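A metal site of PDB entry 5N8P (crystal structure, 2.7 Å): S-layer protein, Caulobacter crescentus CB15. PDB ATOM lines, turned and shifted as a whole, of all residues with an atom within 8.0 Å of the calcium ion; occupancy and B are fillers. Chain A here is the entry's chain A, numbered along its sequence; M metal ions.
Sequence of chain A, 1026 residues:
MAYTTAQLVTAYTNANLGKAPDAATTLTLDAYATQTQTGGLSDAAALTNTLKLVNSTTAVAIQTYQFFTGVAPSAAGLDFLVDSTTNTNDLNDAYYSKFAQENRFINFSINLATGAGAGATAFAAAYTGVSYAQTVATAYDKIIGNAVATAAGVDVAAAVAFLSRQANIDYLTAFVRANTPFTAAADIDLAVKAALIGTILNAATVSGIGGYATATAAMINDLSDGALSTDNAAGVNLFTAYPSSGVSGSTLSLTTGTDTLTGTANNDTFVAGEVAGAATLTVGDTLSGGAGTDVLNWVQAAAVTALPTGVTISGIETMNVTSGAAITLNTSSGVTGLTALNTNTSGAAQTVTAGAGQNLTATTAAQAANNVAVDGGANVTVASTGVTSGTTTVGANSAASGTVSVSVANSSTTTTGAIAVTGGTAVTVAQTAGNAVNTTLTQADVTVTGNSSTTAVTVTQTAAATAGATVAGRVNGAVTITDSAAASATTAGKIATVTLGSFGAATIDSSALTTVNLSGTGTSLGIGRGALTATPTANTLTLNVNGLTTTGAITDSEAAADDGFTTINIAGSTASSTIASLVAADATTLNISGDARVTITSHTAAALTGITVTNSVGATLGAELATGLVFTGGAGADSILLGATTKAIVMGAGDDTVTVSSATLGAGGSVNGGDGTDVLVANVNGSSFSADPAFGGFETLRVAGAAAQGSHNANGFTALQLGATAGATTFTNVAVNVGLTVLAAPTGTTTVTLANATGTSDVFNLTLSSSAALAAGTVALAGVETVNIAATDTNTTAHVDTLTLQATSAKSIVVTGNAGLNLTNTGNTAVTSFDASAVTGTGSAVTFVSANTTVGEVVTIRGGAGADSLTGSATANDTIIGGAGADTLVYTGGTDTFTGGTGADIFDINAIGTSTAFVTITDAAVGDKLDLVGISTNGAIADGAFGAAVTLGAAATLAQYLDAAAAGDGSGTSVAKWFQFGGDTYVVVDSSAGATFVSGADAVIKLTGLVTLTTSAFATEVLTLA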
ATOM      1  N   SER A 770      19.154 -20.238  11.124  1.00  0.00           N
ATOM      2  CA  SER A 770      18.107 -21.115  10.624  1.00  0.00           C
ATOM      3  C   SER A 770      17.187 -21.585  11.746  1.00  0.00           C
ATOM      4  O   SER A 770      17.598 -21.605  12.918  1.00  0.00           O
ATOM      5  CB  SER A 770      18.715 -22.344   9.938  1.00  0.00           C
ATOM      6  OG  SER A 770      19.653 -23.007  10.777  1.00  0.00           O
ATOM      7  N   SER A 771      15.964 -21.970  11.396  1.00  0.00           N
ATOM      8  CA  SER A 771      15.071 -22.613  12.360  1.00  0.00           C
ATOM      9  C   SER A 771      15.439 -24.089  12.546  1.00  0.00           C
ATOM     10  O   SER A 771      15.458 -24.586  13.681  1.00  0.00           O
ATOM     11  CB  SER A 771      13.601 -22.436  11.959  1.00  0.00           C
ATOM     12  OG  SER A 771      13.311 -23.153  10.781  1.00  0.00           O
ATOM     13  N   ALA A 772      15.741 -24.777  11.427  1.00  0.00           N
ATOM     14  CA  ALA A 772      16.174 -26.188  11.422  1.00  0.00           C
ATOM     15  C   ALA A 772      17.705 -26.374  11.236  1.00  0.00           C
ATOM     16  O   ALA A 772      18.434 -25.435  10.860  1.00  0.00           O
ATOM     17  CB  ALA A 772      15.416 -26.949  10.346  1.00  0.00           C
ATOM     18  N   ALA A 773      18.156 -27.609  11.495  1.00  0.00           N
ATOM     19  CA  ALA A 773      19.529 -28.031  11.187  1.00  0.00           C
ATOM     20  C   ALA A 773      19.982 -27.576   9.777  1.00  0.00           C
ATOM     21  O   ALA A 773      19.324 -27.880   8.769  1.00  0.00           O
ATOM     22  CB  ALA A 773      19.670 -29.543  11.370  1.00  0.00           C
ATOM     23  N   THR A 792      23.248 -19.963  15.101  1.00  0.00           N
ATOM     24  CA  THR A 792      21.978 -19.419  15.570  1.00  0.00           C
ATOM     25  C   THR A 792      20.798 -20.297  15.115  1.00  0.00           C
ATOM     26  O   THR A 792      20.704 -20.720  13.930  1.00  0.00           O
ATOM     27  CB  THR A 792      21.842 -17.923  15.195  1.00  0.00           C
ATOM     28  OG1 THR A 792      22.985 -17.219  15.699  1.00  0.00           O
ATOM     29  CG2 THR A 792      20.594 -17.296  15.809  1.00  0.00           C
ATOM     30  N   ASP A 793      19.990 -20.637  16.126  1.00  0.00           N
ATOM     31  CA  ASP A 793      18.663 -21.284  16.013  1.00  0.00           C
ATOM     32  C   ASP A 793      17.625 -20.172  16.197  1.00  0.00           C
ATOM     33  O   ASP A 793      17.695 -19.386  17.154  1.00  0.00           O
ATOM     34  CB  ASP A 793      18.527 -22.362  17.096  1.00  0.00           C
ATOM     35  CG  ASP A 793      17.288 -23.269  16.933  1.00  0.00           C
ATOM     36  OD1 ASP A 793      16.349 -22.996  16.158  1.00  0.00           O
ATOM     37  OD2 ASP A 793      17.258 -24.312  17.607  1.00  0.00           O
ATOM     38  N   THR A 794      16.694 -20.090  15.251  1.00  0.00           N
ATOM     39  CA  THR A 794      15.640 -19.064  15.278  1.00  0.00           C
ATOM     40  C   THR A 794      14.385 -19.508  16.080  1.00  0.00           C
ATOM     41  O   THR A 794      13.627 -18.626  16.557  1.00  0.00           O
ATOM     42  CB  THR A 794      15.268 -18.538  13.854  1.00  0.00           C
ATOM     43  OG1 THR A 794      14.930 -19.629  13.001  1.00  0.00           O
ATOM     44  CG2 THR A 794      16.411 -17.787  13.215  1.00  0.00           C
ATOM     45  N   ASN A 795      14.168 -20.826  16.230  1.00  0.00           N
ATOM     46  CA  ASN A 795      13.083 -21.381  17.090  1.00  0.00           C
ATOM     47  C   ASN A 795      13.567 -22.034  18.404  1.00  0.00           C
ATOM     48  O   ASN A 795      14.757 -22.309  18.593  1.00  0.00           O
ATOM     49  CB  ASN A 795      12.106 -22.298  16.299  1.00  0.00           C
ATOM     50  CG  ASN A 795      12.651 -23.719  16.041  1.00  0.00           C
ATOM     51  OD1 ASN A 795      13.475 -24.246  16.796  1.00  0.00           O
ATOM     52  ND2 ASN A 795      12.165 -24.350  14.981  1.00  0.00           N
ATOM     53  N   THR A 796      12.600 -22.323  19.282  1.00  0.00           N
ATOM     54  CA  THR A 796      12.778 -22.871  20.650  1.00  0.00           C
ATOM     55  C   THR A 796      13.268 -24.326  20.755  1.00  0.00           C
ATOM     56  O   THR A 796      13.679 -24.773  21.837  1.00  0.00           O
ATOM     57  CB  THR A 796      11.438 -22.863  21.414  1.00  0.00           C
ATOM     58  OG1 THR A 796      10.421 -23.452  20.571  1.00  0.00           O
ATOM     59  CG2 THR A 796      11.022 -21.414  21.840  1.00  0.00           C
ATOM     60  N   THR A 797      13.205 -25.076  19.658  1.00  0.00           N
ATOM     61  CA  THR A 797      13.541 -26.493  19.636  1.00  0.00           C
ATOM     62  C   THR A 797      14.985 -26.757  19.078  1.00  0.00           C
ATOM     63  O   THR A 797      15.274 -26.403  17.934  1.00  0.00           O
ATOM     64  CB  THR A 797      12.418 -27.317  18.963  1.00  0.00           C
ATOM     65  OG1 THR A 797      12.969 -28.146  17.936  1.00  0.00           O
ATOM     66  CG2 THR A 797      11.290 -26.404  18.362  1.00  0.00           C
ATOM     67  N   ALA A 798      15.859 -27.364  19.883  1.00  0.00           N
ATOM     68  CA  ALA A 798      17.290 -27.490  19.626  1.00  0.00           C
ATOM     69  C   ALA A 798      17.721 -28.239  18.329  1.00  0.00           C
ATOM     70  O   ALA A 798      17.078 -29.213  17.950  1.00  0.00           O
ATOM     71  CB  ALA A 798      17.987 -28.072  20.860  1.00  0.00           C
ATOM     72  N   HIS A 799      18.791 -27.768  17.669  1.00  0.00           N
ATOM     73  CA  HIS A 799      19.442 -28.459  16.514  1.00  0.00           C
ATOM     74  C   HIS A 799      20.985 -28.275  16.400  1.00  0.00           C
ATOM     75  O   HIS A 799      21.616 -27.462  17.110  1.00  0.00           O
ATOM     76  CB  HIS A 799      18.773 -28.078  15.173  1.00  0.00           C
ATOM     77  CG  HIS A 799      18.927 -26.643  14.764  1.00  0.00           C
ATOM     78  ND1 HIS A 799      19.909 -26.200  13.907  1.00  0.00           N
ATOM     79  CD2 HIS A 799      18.215 -25.537  15.092  1.00  0.00           C
ATOM     80  CE1 HIS A 799      19.790 -24.886  13.728  1.00  0.00           C
ATOM     81  NE2 HIS A 799      18.765 -24.467  14.439  1.00  0.00           N
ATOM     82  N   VAL A 800      21.588 -29.043  15.482  1.00  0.00           N
ATOM     83  CA  VAL A 800      23.023 -29.026  15.243  1.00  0.00           C
ATOM     84  C   VAL A 800      23.365 -28.720  13.777  1.00  0.00           C
ATOM     85  O   VAL A 800      23.034 -29.536  12.896  1.00  0.00           O
ATOM     86  CB  VAL A 800      23.661 -30.394  15.641  1.00  0.00           C
ATOM     87  CG1 VAL A 800      25.185 -30.379  15.450  1.00  0.00           C
ATOM     88  CG2 VAL A 800      23.301 -30.797  17.069  1.00  0.00           C
ATOM     89  N   ASP A 801      24.031 -27.575  13.529  1.00  0.00           N
ATOM     90  CA  ASP A 801      24.458 -27.134  12.177  1.00  0.00           C
ATOM     91  C   ASP A 801      25.756 -27.849  11.749  1.00  0.00           C
ATOM     92  O   ASP A 801      26.506 -28.310  12.611  1.00  0.00           O
ATOM     93  CB  ASP A 801      24.706 -25.616  12.134  1.00  0.00           C
ATOM     94  CG  ASP A 801      23.403 -24.766  12.270  1.00  0.00           C
ATOM     95  OD1 ASP A 801      22.314 -25.207  11.834  1.00  0.00           O
ATOM     96  OD2 ASP A 801      23.472 -23.603  12.784  1.00  0.00           O
ATOM     97  N   ASN A 818      23.568 -20.565  20.002  1.00  0.00           N
ATOM     98  CA  ASN A 818      22.583 -21.339  20.765  1.00  0.00           C
ATOM     99  C   ASN A 818      22.166 -22.548  19.971  1.00  0.00           C
ATOM    100  O   ASN A 818      21.145 -23.150  20.249  1.00  0.00           O
ATOM    101  CB  ASN A 818      21.355 -20.475  21.078  1.00  0.00           C
ATOM    102  CG  ASN A 818      20.715 -19.916  19.841  1.00  0.00           C
ATOM    103  OD1 ASN A 818      19.756 -20.467  19.349  1.00  0.00           O
ATOM    104  ND2 ASN A 818      21.280 -18.831  19.308  1.00  0.00           N
ATOM    105  N   ALA A 819      22.953 -22.905  18.965  1.00  0.00           N
ATOM    106  CA  ALA A 819      22.790 -24.181  18.318  1.00  0.00           C
ATOM    107  C   ALA A 819      24.142 -24.893  18.200  1.00  0.00           C
ATOM    108  O   ALA A 819      25.182 -24.272  18.374  1.00  0.00           O
ATOM    109  CB  ALA A 819      22.126 -24.014  16.984  1.00  0.00           C
HETATM  110 CA    CA M   1      15.574 -25.552  15.746  1.00  0.00          CA
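The backbone carbonyl oxygen of Ser 771 lies close to a ring nitrogen (NE2) of His 799 (3.4 Å). A ring nitrogen (ND1) of His 799 is in hydrogen-bond range of the backbone NH (N) of Ala 773 (3.3 Å). OD1 of Asp 793 lies close to NE2 of His 799, at 3.3 Å. N of Ser 771 lies within hydrogen-bond range of OG1 of Thr 794, 3.0 Å away. A ring nitrogen (ND1) of His 799 sits close to the backbone carbonyl oxygen (O) of Ala 772 (3.5 Å). The side-chain amide oxygen (OD1) of Asn 818 sits close to the backbone carbonyl oxygen (O) of Asp 793. O of Ser 770 lies within hydrogen-bond range of NE2 of His 799 (3.4 Å). A ring nitrogen (ND1) of His 799 lies close to the side-chain carboxylate (OD1) of Asp 801, at 3.3 Å.
CD2 of His 799 touches the calcium ion, 2.7 Å away. Within 4 Å of the calcium ion: Ser 771, Asp 793, Asn 795, Thr 797 and His 799.
O of Ser 771 is bound to the calcium ion, 2.3 Å away. O of Thr 797 binds the calcium ion (2.4 Å). OD1 of Asn 795 binds the calcium ion (2.7 Å). OD1 of Asp 793 binds the calcium ion. The calcium ion is bound by the side-chain carboxylate (OD2) of Asp 793, 2.8 Å away.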
